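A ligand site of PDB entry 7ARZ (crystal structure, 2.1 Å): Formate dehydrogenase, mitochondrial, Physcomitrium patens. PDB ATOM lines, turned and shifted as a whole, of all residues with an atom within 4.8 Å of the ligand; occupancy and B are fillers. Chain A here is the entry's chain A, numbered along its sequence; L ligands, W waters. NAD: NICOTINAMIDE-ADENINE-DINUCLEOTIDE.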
ATOM      1  N   PHE A  80     -29.061 -29.115 -35.599  1.00  0.00           N
ATOM      2  CA  PHE A  80     -30.323 -29.395 -34.850  1.00  0.00           C
ATOM      3  C   PHE A  80     -30.945 -30.686 -35.375  1.00  0.00           C
ATOM      4  O   PHE A  80     -31.845 -31.263 -34.705  1.00  0.00           O
ATOM      5  CB  PHE A  80     -31.236 -28.167 -34.913  1.00  0.00           C
ATOM      6  CG  PHE A  80     -30.431 -26.900 -34.871  1.00  0.00           C
ATOM      7  CD1 PHE A  80     -29.710 -26.567 -33.742  1.00  0.00           C
ATOM      8  CD2 PHE A  80     -30.276 -26.100 -36.009  1.00  0.00           C
ATOM      9  CE1 PHE A  80     -28.891 -25.441 -33.705  1.00  0.00           C
ATOM     10  CE2 PHE A  80     -29.446 -24.983 -35.970  1.00  0.00           C
ATOM     11  CZ  PHE A  80     -28.756 -24.651 -34.822  1.00  0.00           C
ATOM     12  N   VAL A 104     -23.650 -23.637 -36.189  1.00  0.00           N
ATOM     13  CA  VAL A 104     -22.241 -23.653 -35.703  1.00  0.00           C
ATOM     14  C   VAL A 104     -21.946 -25.018 -35.077  1.00  0.00           C
ATOM     15  O   VAL A 104     -22.789 -25.500 -34.302  1.00  0.00           O
ATOM     16  CB  VAL A 104     -22.053 -22.521 -34.693  1.00  0.00           C
ATOM     17  CG1 VAL A 104     -20.650 -22.519 -34.103  1.00  0.00           C
ATOM     18  CG2 VAL A 104     -22.391 -21.186 -35.321  1.00  0.00           C
ATOM     19  N   GLY A 105     -20.774 -25.594 -35.397  1.00  0.00           N
ATOM     20  CA  GLY A 105     -20.402 -26.973 -35.063  1.00  0.00           C
ATOM     21  C   GLY A 105     -20.641 -27.921 -36.229  1.00  0.00           C
ATOM     22  O   GLY A 105     -21.818 -28.198 -36.590  1.00  0.00           O
ATOM     23  N   ASP A 107     -19.065 -31.053 -36.427  1.00  0.00           N
ATOM     24  CA  ASP A 107     -18.591 -32.359 -35.899  1.00  0.00           C
ATOM     25  C   ASP A 107     -19.428 -33.512 -36.447  1.00  0.00           C
ATOM     26  O   ASP A 107     -18.938 -34.639 -36.368  1.00  0.00           O
ATOM     27  CB  ASP A 107     -18.628 -32.399 -34.358  1.00  0.00           C
ATOM     28  CG  ASP A 107     -19.890 -31.748 -33.835  1.00  0.00           C
ATOM     29  OD1 ASP A 107     -19.863 -30.502 -33.716  1.00  0.00           O
ATOM     30  OD2 ASP A 107     -20.926 -32.463 -33.684  1.00  0.00           O
ATOM     31  N   ASN A 128     -24.978 -17.656 -33.801  1.00  0.00           N
ATOM     32  CA  ASN A 128     -25.939 -18.013 -32.716  1.00  0.00           C
ATOM     33  C   ASN A 128     -25.166 -18.175 -31.412  1.00  0.00           C
ATOM     34  O   ASN A 128     -25.674 -18.867 -30.496  1.00  0.00           O
ATOM     35  CB  ASN A 128     -26.779 -19.253 -33.060  1.00  0.00           C
ATOM     36  CG  ASN A 128     -25.939 -20.462 -33.421  1.00  0.00           C
ATOM     37  OD1 ASN A 128     -24.727 -20.473 -33.170  1.00  0.00           O
ATOM     38  ND2 ASN A 128     -26.565 -21.465 -34.014  1.00  0.00           N
ATOM     39  N   VAL A 129     -24.051 -17.473 -31.308  1.00  0.00           N
ATOM     40  CA  VAL A 129     -23.116 -17.538 -30.163  1.00  0.00           C
ATOM     41  C   VAL A 129     -23.687 -16.687 -29.031  1.00  0.00           C
ATOM     42  O   VAL A 129     -23.545 -17.109 -27.860  1.00  0.00           O
ATOM     43  CB  VAL A 129     -21.689 -17.158 -30.587  1.00  0.00           C
ATOM     44  CG1 VAL A 129     -21.229 -18.033 -31.725  1.00  0.00           C
ATOM     45  CG2 VAL A 129     -21.541 -15.690 -30.977  1.00  0.00           C
ATOM     46  N   VAL A 132     -26.842 -18.942 -27.602  1.00  0.00           N
ATOM     47  CA  VAL A 132     -26.361 -20.044 -26.723  1.00  0.00           C
ATOM     48  C   VAL A 132     -25.858 -19.468 -25.403  1.00  0.00           C
ATOM     49  O   VAL A 132     -26.108 -20.099 -24.374  1.00  0.00           O
ATOM     50  CB  VAL A 132     -25.281 -20.884 -27.410  1.00  0.00           C
ATOM     51  CG1 VAL A 132     -24.768 -21.974 -26.480  1.00  0.00           C
ATOM     52  CG2 VAL A 132     -25.790 -21.494 -28.693  1.00  0.00           C
ATOM     53  N   GLY A 180     -13.544 -23.448 -22.413  1.00  0.00           N
ATOM     54  CA  GLY A 180     -13.618 -22.746 -23.702  1.00  0.00           C
ATOM     55  C   GLY A 180     -13.843 -21.266 -23.479  1.00  0.00           C
ATOM     56  O   GLY A 180     -14.746 -20.921 -22.672  1.00  0.00           O
ATOM     57  N   GLY A 181     -13.021 -20.443 -24.112  1.00  0.00           N
ATOM     58  CA  GLY A 181     -13.018 -18.970 -24.001  1.00  0.00           C
ATOM     59  C   GLY A 181     -13.177 -18.406 -25.372  1.00  0.00           C
ATOM     60  O   GLY A 181     -12.589 -17.350 -25.666  1.00  0.00           O
ATOM     61  N   GLY A 182     -13.911 -19.140 -26.222  1.00  0.00           N
ATOM     62  CA  GLY A 182     -14.192 -18.760 -27.613  1.00  0.00           C
ATOM     63  C   GLY A 182     -15.301 -17.733 -27.642  1.00  0.00           C
ATOM     64  O   GLY A 182     -15.440 -16.993 -26.666  1.00  0.00           O
ATOM     65  N   ARG A 183     -16.094 -17.721 -28.725  1.00  0.00           N
ATOM     66  CA  ARG A 183     -17.176 -16.742 -28.940  1.00  0.00           C
ATOM     67  C   ARG A 183     -18.232 -16.957 -27.848  1.00  0.00           C
ATOM     68  O   ARG A 183     -18.626 -15.944 -27.253  1.00  0.00           O
ATOM     69  CB  ARG A 183     -17.710 -16.867 -30.367  1.00  0.00           C
ATOM     70  CG  ARG A 183     -16.694 -16.426 -31.419  1.00  0.00           C
ATOM     71  CD  ARG A 183     -17.051 -16.825 -32.832  1.00  0.00           C
ATOM     72  NE  ARG A 183     -16.056 -16.352 -33.787  1.00  0.00           N
ATOM     73  CZ  ARG A 183     -14.889 -16.950 -34.064  1.00  0.00           C
ATOM     74  NH1 ARG A 183     -14.523 -18.089 -33.482  1.00  0.00           N
ATOM     75  NH2 ARG A 183     -14.068 -16.399 -34.944  1.00  0.00           N
ATOM     76  N   ILE A 184     -18.679 -18.193 -27.598  1.00  0.00           N
ATOM     77  CA  ILE A 184     -19.765 -18.461 -26.618  1.00  0.00           C
ATOM     78  C   ILE A 184     -19.219 -18.256 -25.196  1.00  0.00           C
ATOM     79  O   ILE A 184     -19.820 -17.460 -24.438  1.00  0.00           O
ATOM     80  CB  ILE A 184     -20.404 -19.852 -26.834  1.00  0.00           C
ATOM     81  CG1 ILE A 184     -20.894 -20.026 -28.276  1.00  0.00           C
ATOM     82  CG2 ILE A 184     -21.560 -20.037 -25.856  1.00  0.00           C
ATOM     83  CD1 ILE A 184     -21.663 -21.324 -28.541  1.00  0.00           C
ATOM     84  N   GLY A 185     -18.080 -18.866 -24.849  1.00  0.00           N
ATOM     85  CA  GLY A 185     -17.362 -18.609 -23.588  1.00  0.00           C
ATOM     86  C   GLY A 185     -17.378 -17.132 -23.216  1.00  0.00           C
ATOM     87  O   GLY A 185     -17.771 -16.803 -22.083  1.00  0.00           O
ATOM     88  N   TYR A 203     -10.908 -21.728 -19.173  1.00  0.00           N
ATOM     89  CA  TYR A 203      -9.838 -22.610 -19.681  1.00  0.00           C
ATOM     90  C   TYR A 203      -9.972 -22.662 -21.199  1.00  0.00           C
ATOM     91  O   TYR A 203     -11.085 -22.941 -21.732  1.00  0.00           O
ATOM     92  CB  TYR A 203      -9.946 -23.980 -19.017  1.00  0.00           C
ATOM     93  CG  TYR A 203      -9.065 -25.056 -19.583  1.00  0.00           C
ATOM     94  CD1 TYR A 203      -7.774 -25.273 -19.100  1.00  0.00           C
ATOM     95  CD2 TYR A 203      -9.531 -25.907 -20.564  1.00  0.00           C
ATOM     96  CE1 TYR A 203      -6.979 -26.291 -19.618  1.00  0.00           C
ATOM     97  CE2 TYR A 203      -8.759 -26.932 -21.083  1.00  0.00           C
ATOM     98  CZ  TYR A 203      -7.472 -27.120 -20.610  1.00  0.00           C
ATOM     99  OH  TYR A 203      -6.724 -28.151 -21.130  1.00  0.00           O
ATOM    100  N   ASP A 204      -8.868 -22.342 -21.875  1.00  0.00           N
ATOM    101  CA  ASP A 204      -8.723 -22.352 -23.356  1.00  0.00           C
ATOM    102  C   ASP A 204      -7.235 -22.528 -23.658  1.00  0.00           C
ATOM    103  O   ASP A 204      -6.422 -22.143 -22.796  1.00  0.00           O
ATOM    104  CB  ASP A 204      -9.292 -21.060 -23.961  1.00  0.00           C
ATOM    105  CG  ASP A 204      -9.757 -21.215 -25.410  1.00  0.00           C
ATOM    106  OD1 ASP A 204      -8.888 -21.235 -26.309  1.00  0.00           O
ATOM    107  OD2 ASP A 204     -10.975 -21.328 -25.605  1.00  0.00           O
ATOM    108  N   ARG A 205      -6.890 -23.088 -24.815  1.00  0.00           N
ATOM    109  CA  ARG A 205      -5.487 -23.118 -25.323  1.00  0.00           C
ATOM    110  C   ARG A 205      -4.990 -21.676 -25.497  1.00  0.00           C
ATOM    111  O   ARG A 205      -3.776 -21.443 -25.366  1.00  0.00           O
ATOM    112  CB  ARG A 205      -5.406 -23.941 -26.618  1.00  0.00           C
ATOM    113  CG  ARG A 205      -5.660 -25.426 -26.390  1.00  0.00           C
ATOM    114  CD  ARG A 205      -5.143 -26.309 -27.517  1.00  0.00           C
ATOM    115  NE  ARG A 205      -5.958 -26.150 -28.717  1.00  0.00           N
ATOM    116  CZ  ARG A 205      -6.524 -27.138 -29.405  1.00  0.00           C
ATOM    117  NH1 ARG A 205      -6.366 -28.405 -29.042  1.00  0.00           N
ATOM    118  NH2 ARG A 205      -7.252 -26.856 -30.479  1.00  0.00           N
ATOM    119  N   ASN A 206      -5.900 -20.723 -25.721  1.00  0.00           N
ATOM    120  CA  ASN A 206      -5.578 -19.319 -26.088  1.00  0.00           C
ATOM    121  C   ASN A 206      -5.945 -18.365 -24.956  1.00  0.00           C
ATOM    122  O   ASN A 206      -7.140 -18.262 -24.609  1.00  0.00           O
ATOM    123  CB  ASN A 206      -6.274 -18.909 -27.402  1.00  0.00           C
ATOM    124  CG  ASN A 206      -5.834 -19.768 -28.571  1.00  0.00           C
ATOM    125  OD1 ASN A 206      -6.656 -20.364 -29.264  1.00  0.00           O
ATOM    126  ND2 ASN A 206      -4.525 -19.847 -28.770  1.00  0.00           N
ATOM    127  N   ASN A 237     -17.877 -25.108 -23.412  1.00  0.00           N
ATOM    128  CA  ASN A 237     -17.909 -24.143 -24.551  1.00  0.00           C
ATOM    129  C   ASN A 237     -16.750 -24.413 -25.523  1.00  0.00           C
ATOM    130  O   ASN A 237     -16.133 -23.435 -25.980  1.00  0.00           O
ATOM    131  CB  ASN A 237     -17.923 -22.693 -24.063  1.00  0.00           C
ATOM    132  CG  ASN A 237     -19.316 -22.232 -23.673  1.00  0.00           C
ATOM    133  OD1 ASN A 237     -20.281 -22.582 -24.327  1.00  0.00           O
ATOM    134  ND2 ASN A 237     -19.421 -21.481 -22.596  1.00  0.00           N
ATOM    135  N   THR A 238     -16.493 -25.687 -25.827  1.00  0.00           N
ATOM    136  CA  THR A 238     -15.538 -26.128 -26.887  1.00  0.00           C
ATOM    137  C   THR A 238     -16.319 -26.760 -28.030  1.00  0.00           C
ATOM    138  O   THR A 238     -17.454 -27.211 -27.859  1.00  0.00           O
ATOM    139  CB  THR A 238     -14.508 -27.140 -26.382  1.00  0.00           C
ATOM    140  OG1 THR A 238     -15.205 -28.325 -25.981  1.00  0.00           O
ATOM    141  CG2 THR A 238     -13.666 -26.635 -25.227  1.00  0.00           C
ATOM    142  N   PRO A 239     -15.714 -26.875 -29.240  1.00  0.00           N
ATOM    143  CA  PRO A 239     -16.265 -27.747 -30.268  1.00  0.00           C
ATOM    144  C   PRO A 239     -16.070 -29.173 -29.765  1.00  0.00           C
ATOM    145  O   PRO A 239     -15.318 -29.346 -28.832  1.00  0.00           O
ATOM    146  CB  PRO A 239     -15.451 -27.438 -31.531  1.00  0.00           C
ATOM    147  CG  PRO A 239     -14.580 -26.236 -31.176  1.00  0.00           C
ATOM    148  CD  PRO A 239     -14.465 -26.220 -29.664  1.00  0.00           C
ATOM    149  N   LEU A 240     -16.750 -30.131 -30.364  1.00  0.00           N
ATOM    150  CA  LEU A 240     -16.461 -31.571 -30.216  1.00  0.00           C
ATOM    151  C   LEU A 240     -15.306 -31.942 -31.161  1.00  0.00           C
ATOM    152  O   LEU A 240     -15.567 -32.083 -32.370  1.00  0.00           O
ATOM    153  CB  LEU A 240     -17.723 -32.374 -30.565  1.00  0.00           C
ATOM    154  CG  LEU A 240     -17.515 -33.878 -30.568  1.00  0.00           C
ATOM    155  CD1 LEU A 240     -17.053 -34.329 -29.190  1.00  0.00           C
ATOM    156  CD2 LEU A 240     -18.765 -34.613 -31.019  1.00  0.00           C
ATOM    157  N   THR A 241     -14.087 -32.048 -30.626  1.00  0.00           N
ATOM    158  CA  THR A 241     -12.835 -32.497 -31.296  1.00  0.00           C
ATOM    159  C   THR A 241     -12.407 -33.856 -30.739  1.00  0.00           C
ATOM    160  O   THR A 241     -13.177 -34.436 -29.947  1.00  0.00           O
ATOM    161  CB  THR A 241     -11.739 -31.443 -31.151  1.00  0.00           C
ATOM    162  OG1 THR A 241     -11.071 -31.559 -29.886  1.00  0.00           O
ATOM    163  CG2 THR A 241     -12.308 -30.044 -31.308  1.00  0.00           C
ATOM    164  N   GLN A 243      -9.544 -34.231 -28.936  1.00  0.00           N
ATOM    165  CA  GLN A 243      -9.240 -33.725 -27.575  1.00  0.00           C
ATOM    166  C   GLN A 243     -10.492 -33.701 -26.673  1.00  0.00           C
ATOM    167  O   GLN A 243     -10.331 -33.996 -25.474  1.00  0.00           O
ATOM    168  CB  GLN A 243      -8.724 -32.285 -27.620  1.00  0.00           C
ATOM    169  CG  GLN A 243      -7.747 -31.993 -28.750  1.00  0.00           C
ATOM    170  CD  GLN A 243      -6.579 -32.940 -28.808  1.00  0.00           C
ATOM    171  OE1 GLN A 243      -5.829 -33.098 -27.839  1.00  0.00           O
ATOM    172  NE2 GLN A 243      -6.421 -33.580 -29.951  1.00  0.00           N
ATOM    173  N   THR A 244     -11.689 -33.328 -27.173  1.00  0.00           N
ATOM    174  CA  THR A 244     -12.823 -32.949 -26.278  1.00  0.00           C
ATOM    175  C   THR A 244     -13.891 -34.038 -26.199  1.00  0.00           C
ATOM    176  O   THR A 244     -14.690 -33.960 -25.249  1.00  0.00           O
ATOM    177  CB  THR A 244     -13.539 -31.651 -26.666  1.00  0.00           C
ATOM    178  OG1 THR A 244     -14.187 -31.823 -27.927  1.00  0.00           O
ATOM    179  CG2 THR A 244     -12.624 -30.449 -26.690  1.00  0.00           C
ATOM    180  N   ASN A 265     -24.306 -26.816 -23.626  1.00  0.00           N
ATOM    181  CA  ASN A 265     -24.991 -26.455 -24.908  1.00  0.00           C
ATOM    182  C   ASN A 265     -23.964 -26.462 -26.060  1.00  0.00           C
ATOM    183  O   ASN A 265     -24.227 -25.824 -27.116  1.00  0.00           O
ATOM    184  CB  ASN A 265     -25.653 -25.069 -24.829  1.00  0.00           C
ATOM    185  CG  ASN A 265     -26.942 -25.042 -24.057  1.00  0.00           C
ATOM    186  OD1 ASN A 265     -27.167 -25.850 -23.165  1.00  0.00           O
ATOM    187  ND2 ASN A 265     -27.821 -24.114 -24.406  1.00  0.00           N
ATOM    188  N   ALA A 266     -22.811 -27.111 -25.859  1.00  0.00           N
ATOM    189  CA  ALA A 266     -21.743 -27.295 -26.870  1.00  0.00           C
ATOM    190  C   ALA A 266     -22.091 -28.540 -27.692  1.00  0.00           C
ATOM    191  O   ALA A 266     -22.798 -28.390 -28.692  1.00  0.00           O
ATOM    192  CB  ALA A 266     -20.371 -27.357 -26.228  1.00  0.00           C
ATOM    193  N   ARG A 267     -21.685 -29.725 -27.225  1.00  0.00           N
ATOM    194  CA  ARG A 267     -22.020 -31.019 -27.873  1.00  0.00           C
ATOM    195  C   ARG A 267     -22.103 -32.123 -26.812  1.00  0.00           C
ATOM    196  O   ARG A 267     -21.223 -32.207 -25.967  1.00  0.00           O
ATOM    197  CB  ARG A 267     -20.954 -31.356 -28.925  1.00  0.00           C
ATOM    198  CG  ARG A 267     -20.984 -30.483 -30.164  1.00  0.00           C
ATOM    199  CD  ARG A 267     -22.281 -30.702 -30.912  1.00  0.00           C
ATOM    200  NE  ARG A 267     -22.409 -30.020 -32.190  1.00  0.00           N
ATOM    201  CZ  ARG A 267     -22.824 -28.762 -32.378  1.00  0.00           C
ATOM    202  NH1 ARG A 267     -23.132 -27.986 -31.351  1.00  0.00           N
ATOM    203  NH2 ARG A 267     -22.977 -28.306 -33.615  1.00  0.00           N
ATOM    204  N   ASP A 291     -28.980 -28.584 -24.266  1.00  0.00           N
ATOM    205  CA  ASP A 291     -29.869 -28.843 -25.417  1.00  0.00           C
ATOM    206  C   ASP A 291     -29.222 -29.896 -26.327  1.00  0.00           C
ATOM    207  O   ASP A 291     -29.917 -30.365 -27.218  1.00  0.00           O
ATOM    208  CB  ASP A 291     -30.213 -27.542 -26.150  1.00  0.00           C
ATOM    209  CG  ASP A 291     -29.018 -26.778 -26.691  1.00  0.00           C
ATOM    210  OD1 ASP A 291     -27.903 -26.955 -26.151  1.00  0.00           O
ATOM    211  OD2 ASP A 291     -29.219 -25.997 -27.659  1.00  0.00           O
ATOM    212  N   VAL A 292     -27.969 -30.291 -26.070  1.00  0.00           N
ATOM    213  CA  VAL A 292     -27.193 -31.126 -27.027  1.00  0.00           C
ATOM    214  C   VAL A 292     -26.978 -32.556 -26.487  1.00  0.00           C
ATOM    215  O   VAL A 292     -26.775 -32.730 -25.277  1.00  0.00           O
ATOM    216  CB  VAL A 292     -25.874 -30.439 -27.441  1.00  0.00           C
ATOM    217  CG1 VAL A 292     -26.161 -29.249 -28.347  1.00  0.00           C
ATOM    218  CG2 VAL A 292     -25.020 -30.035 -26.244  1.00  0.00           C
ATOM    219  N   HIS A 315     -32.318 -29.929 -29.016  1.00  0.00           N
ATOM    220  CA  HIS A 315     -31.326 -28.960 -29.526  1.00  0.00           C
ATOM    221  C   HIS A 315     -32.055 -27.716 -30.039  1.00  0.00           C
ATOM    222  O   HIS A 315     -32.462 -27.711 -31.245  1.00  0.00           O
ATOM    223  CB  HIS A 315     -30.444 -29.663 -30.547  1.00  0.00           C
ATOM    224  CG  HIS A 315     -29.235 -28.872 -30.939  1.00  0.00           C
ATOM    225  ND1 HIS A 315     -28.298 -29.388 -31.819  1.00  0.00           N
ATOM    226  CD2 HIS A 315     -28.818 -27.635 -30.609  1.00  0.00           C
ATOM    227  CE1 HIS A 315     -27.320 -28.496 -31.956  1.00  0.00           C
ATOM    228  NE2 HIS A 315     -27.631 -27.409 -31.246  1.00  0.00           N
ATOM    229  N   SER A 317     -31.212 -24.144 -28.570  1.00  0.00           N
ATOM    230  CA  SER A 317     -30.712 -22.806 -28.162  1.00  0.00           C
ATOM    231  C   SER A 317     -30.194 -22.033 -29.381  1.00  0.00           C
ATOM    232  O   SER A 317     -30.434 -20.814 -29.455  1.00  0.00           O
ATOM    233  CB  SER A 317     -29.706 -22.876 -27.040  1.00  0.00           C
ATOM    234  OG  SER A 317     -28.546 -23.546 -27.441  1.00  0.00           O
ATOM    235  N   GLY A 318     -29.508 -22.705 -30.310  1.00  0.00           N
ATOM    236  CA  GLY A 318     -28.886 -22.044 -31.472  1.00  0.00           C
ATOM    237  C   GLY A 318     -29.832 -21.932 -32.664  1.00  0.00           C
ATOM    238  O   GLY A 318     -29.326 -21.590 -33.737  1.00  0.00           O
ATOM    239  N   GLN A 359      -9.055 -24.771 -33.996  1.00  0.00           N
ATOM    240  CA  GLN A 359      -9.951 -25.051 -32.847  1.00  0.00           C
ATOM    241  C   GLN A 359     -10.553 -26.460 -32.952  1.00  0.00           C
ATOM    242  O   GLN A 359     -11.206 -26.837 -31.972  1.00  0.00           O
ATOM    243  CB  GLN A 359     -11.029 -23.958 -32.679  1.00  0.00           C
ATOM    244  CG  GLN A 359     -12.224 -24.081 -33.624  1.00  0.00           C
ATOM    245  CD  GLN A 359     -12.066 -23.285 -34.897  1.00  0.00           C
ATOM    246  OE1 GLN A 359     -10.968 -22.921 -35.299  1.00  0.00           O
ATOM    247  NE2 GLN A 359     -13.188 -22.975 -35.544  1.00  0.00           N
ATOM    248  N   TYR A 360     -10.331 -27.216 -34.042  1.00  0.00           N
ATOM    249  CA  TYR A 360     -10.788 -28.641 -34.172  1.00  0.00           C
ATOM    250  C   TYR A 360      -9.601 -29.615 -34.035  1.00  0.00           C
ATOM    251  O   TYR A 360      -9.828 -30.852 -34.019  1.00  0.00           O
ATOM    252  CB  TYR A 360     -11.598 -28.848 -35.464  1.00  0.00           C
ATOM    253  CG  TYR A 360     -13.060 -28.475 -35.349  1.00  0.00           C
ATOM    254  CD1 TYR A 360     -13.454 -27.155 -35.362  1.00  0.00           C
ATOM    255  CD2 TYR A 360     -14.059 -29.440 -35.224  1.00  0.00           C
ATOM    256  CE1 TYR A 360     -14.782 -26.776 -35.239  1.00  0.00           C
ATOM    257  CE2 TYR A 360     -15.390 -29.084 -35.085  1.00  0.00           C
ATOM    258  CZ  TYR A 360     -15.761 -27.744 -35.076  1.00  0.00           C
ATOM    259  OH  TYR A 360     -17.070 -27.328 -34.947  1.00  0.00           O
ATOM    260  N   LEU A 361      -8.386 -29.085 -33.865  1.00  0.00           N
ATOM    261  CA  LEU A 361      -7.145 -29.857 -33.566  1.00  0.00           C
ATOM    262  C   LEU A 361      -7.035 -30.083 -32.061  1.00  0.00           C
ATOM    263  O   LEU A 361      -8.012 -30.079 -31.296  1.00  0.00           O
ATOM    264  CB  LEU A 361      -5.929 -29.072 -34.057  1.00  0.00           C
ATOM    265  CG  LEU A 361      -5.917 -28.753 -35.551  1.00  0.00           C
ATOM    266  CD1 LEU A 361      -4.646 -27.974 -35.925  1.00  0.00           C
ATOM    267  CD2 LEU A 361      -6.040 -30.028 -36.392  1.00  0.00           C
ATOM    268  OXT LEU A 361      -5.909 -30.268 -31.599  1.00  0.00           O
HETATM  269  PA  NAD L   1     -15.153 -20.873 -30.959  1.00  0.00           P
HETATM  270  O1A NAD L   1     -14.364 -21.603 -31.998  1.00  0.00           O
HETATM  271  O2A NAD L   1     -15.133 -19.375 -30.976  1.00  0.00           O
HETATM  272  O5B NAD L   1     -14.710 -21.346 -29.488  1.00  0.00           O
HETATM  273  C5B NAD L   1     -14.156 -22.654 -29.196  1.00  0.00           C
HETATM  274  C4B NAD L   1     -12.968 -22.500 -28.281  1.00  0.00           C
HETATM  275  O4B NAD L   1     -12.552 -23.823 -27.854  1.00  0.00           O
HETATM  276  C3B NAD L   1     -11.717 -21.835 -28.897  1.00  0.00           C
HETATM  277  O3B NAD L   1     -11.377 -20.648 -28.178  1.00  0.00           O
HETATM  278  C2B NAD L   1     -10.636 -22.929 -28.859  1.00  0.00           C
HETATM  279  O2B NAD L   1      -9.335 -22.508 -28.542  1.00  0.00           O
HETATM  280  C1B NAD L   1     -11.144 -23.814 -27.733  1.00  0.00           C
HETATM  281  N9A NAD L   1     -10.670 -25.187 -27.761  1.00  0.00           N
HETATM  282  C8A NAD L   1     -10.861 -26.148 -28.718  1.00  0.00           C
HETATM  283  N7A NAD L   1     -10.338 -27.314 -28.407  1.00  0.00           N
HETATM  284  C5A NAD L   1      -9.773 -27.099 -27.161  1.00  0.00           C
HETATM  285  C6A NAD L   1      -9.059 -27.940 -26.282  1.00  0.00           C
HETATM  286  N6A NAD L   1      -8.787 -29.212 -26.543  1.00  0.00           N
HETATM  287  N1A NAD L   1      -8.646 -27.406 -25.108  1.00  0.00           N
HETATM  288  C2A NAD L   1      -8.911 -26.126 -24.847  1.00  0.00           C
HETATM  289  N3A NAD L   1      -9.567 -25.228 -25.591  1.00  0.00           N
HETATM  290  C4A NAD L   1      -9.978 -25.790 -26.742  1.00  0.00           C
HETATM  291  O3  NAD L   1     -16.647 -21.458 -31.080  1.00  0.00           O
HETATM  292  PN  NAD L   1     -18.006 -21.063 -30.357  1.00  0.00           P
HETATM  293  O1N NAD L   1     -17.587 -20.598 -29.001  1.00  0.00           O
HETATM  294  O2N NAD L   1     -18.779 -20.147 -31.223  1.00  0.00           O
HETATM  295  O5D NAD L   1     -18.785 -22.454 -30.312  1.00  0.00           O
HETATM  296  C5D NAD L   1     -18.334 -23.533 -29.479  1.00  0.00           C
HETATM  297  C4D NAD L   1     -19.092 -24.775 -29.839  1.00  0.00           C
HETATM  298  O4D NAD L   1     -20.440 -24.650 -29.368  1.00  0.00           O
HETATM  299  C3D NAD L   1     -19.249 -25.120 -31.327  1.00  0.00           C
HETATM  300  O3D NAD L   1     -18.092 -25.774 -31.835  1.00  0.00           O
HETATM  301  C2D NAD L   1     -20.492 -26.014 -31.293  1.00  0.00           C
HETATM  302  O2D NAD L   1     -20.059 -27.352 -31.106  1.00  0.00           O
HETATM  303  C1D NAD L   1     -21.305 -25.547 -30.076  1.00  0.00           C
HETATM  304  N1N NAD L   1     -22.550 -24.784 -30.417  1.00  0.00           N
HETATM  305  C2N NAD L   1     -23.819 -25.255 -30.090  1.00  0.00           C
HETATM  306  C3N NAD L   1     -24.952 -24.494 -30.389  1.00  0.00           C
HETATM  307  C7N NAD L   1     -26.346 -24.926 -29.974  1.00  0.00           C
HETATM  308  O7N NAD L   1     -27.317 -24.701 -30.698  1.00  0.00           O
HETATM  309  N7N NAD L   1     -26.467 -25.545 -28.802  1.00  0.00           N
HETATM  310  C4N NAD L   1     -24.784 -23.328 -31.108  1.00  0.00           C
HETATM  311  C5N NAD L   1     -23.523 -22.799 -31.268  1.00  0.00           C
HETATM  312  C6N NAD L   1     -22.423 -23.597 -31.033  1.00  0.00           C
HETATM  313  O   HOH W   1      -7.895 -24.308 -30.255  1.00  0.00           O
HETATM  314  O   HOH W   2     -17.353 -24.789 -34.415  1.00  0.00           O
HETATM  315  O   HOH W   3     -18.346 -28.831 -32.593  1.00  0.00           O
HETATM  316  O   HOH W   4     -16.259 -20.733 -26.597  1.00  0.00           O
HETATM  317  O   HOH W   5     -12.375 -17.873 -30.668  1.00  0.00           O
HETATM  318  O   HOH W   6     -15.623 -23.038 -34.155  1.00  0.00           O
HETATM  319  O   HOH W   7     -18.922 -19.473 -33.864  1.00  0.00           O
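Water W3 lies within hydrogen-bond range of the side-chain carboxylate of Asp 107, an oxygen (O2D) of the ligand, the backbone NH of Leu 240 and the side-chain hydroxyl of Tyr 360. Water W4 lies within hydrogen-bond range of an oxygen (O1N) of the ligand (2.7 Å), the backbone carbonyl oxygen (O) of Asn 237 (2.8 Å), the backbone NH (N) of Gly 182 (2.9 Å) and the backbone NH (N) of Gly 185 (3.1 Å). Water W2 lies within hydrogen-bond range of OH of Tyr 360 (2.6 Å) and O3D of the ligand (2.9 Å). Water W1 lies within hydrogen-bond range of NH2 of Arg 205 (2.6 Å) and O2B of the ligand (2.9 Å). Water W6 bridges NE2 of Gln 359 (2.8 Å) and O1A of the ligand (2.9 Å).
The side-chain carboxylate (OD2) of Asp 291 sits at hydrogen-bond distance from the side-chain hydroxyl (OG) of Ser 317, 2.6 Å away. The guanidinium group (NH1) of Arg 205 is in salt-bridge range of the chain-end carboxylate (OXT) of Leu 361, 3.2 Å away. O of Tyr 203 lies within hydrogen-bond range of N of Gly 180, at 2.6 Å. The guanidinium group (NE) of Arg 267 lies within salt-bridge range of the side-chain carboxylate (OD1) of Asp 107 (3.0 Å). The guanidinium group (NH2) of Arg 267 lies within hydrogen-bond range of the backbone carbonyl oxygen (O) of Gly 105 (3.2 Å). The backbone carbonyl oxygen (O) of Val 104 is in hydrogen-bond range of the guanidinium group (NH2) of Arg 267 (2.9 Å). OG1 of Thr 241 sits at hydrogen-bond distance from N of Gln 243 (3.2 Å). ND2 of Asn 265 sits at hydrogen-bond distance from OG of Ser 317, at 3.2 Å.
Merely in contact with the ligand: Phe 80 (3.5 Å), Val 104 (3.7 Å), Gly 105 (3.9 Å), Asn 128 (3.2 Å), Val 129 (3.3 Å), Val 132 (3.2 Å), Gly 182 (3.2 Å), Tyr 203 (3.9 Å), Arg 205 (3.5 Å), Asn 206 (3.5 Å), Asn 237 (3.9 Å), Thr 238 (3.5 Å), Pro 239 (3.1 Å), Gln 243 (3.3 Å), Ala 266 (3.5 Å), Val 292 (3.7 Å), Gln 359 (3.3 Å) and Tyr 360 (3.6 Å). Hydrophobic or aromatic side chains within 4 Å of the ligand: Phe 80, Val 104, Val 129, Val 132, Ile 184, Tyr 203, Pro 239, Val 292 and His 315. Of the 35 residues printed, 27 come within 4 Å of the ligand.
N of Gly 318 sits at hydrogen-bond distance from O7N of the ligand. The side-chain carboxylate (OD1) of Asp 204 sits at hydrogen-bond distance from an oxygen (O2B) of the ligand (2.6 Å). A ring nitrogen (NE2) of His 315 lies within hydrogen-bond range of an oxygen (O7N) of the ligand, at 2.8 Å. O2D of the ligand sits close to NH1 of Arg 267 (3.1 Å). NH1 of Arg 183 is in salt-bridge range of O2A of the ligand (2.9 Å). OD2 of Asp 291 is in hydrogen-bond range of N7N of the ligand (3.0 Å). The side-chain hydroxyl (OG) of Ser 317 lies within hydrogen-bond range of a nitrogen (N7N) of the ligand, 3.2 Å away. The backbone carbonyl oxygen (O) of Asn 265 is in hydrogen-bond range of a nitrogen (N7N) of the ligand (2.8 Å). An oxygen (O2A) of the ligand lies within hydrogen-bond range of the backbone NH (N) of Arg 183. N of Ile 184 lies within hydrogen-bond range of O1N of the ligand, 3.0 Å away.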
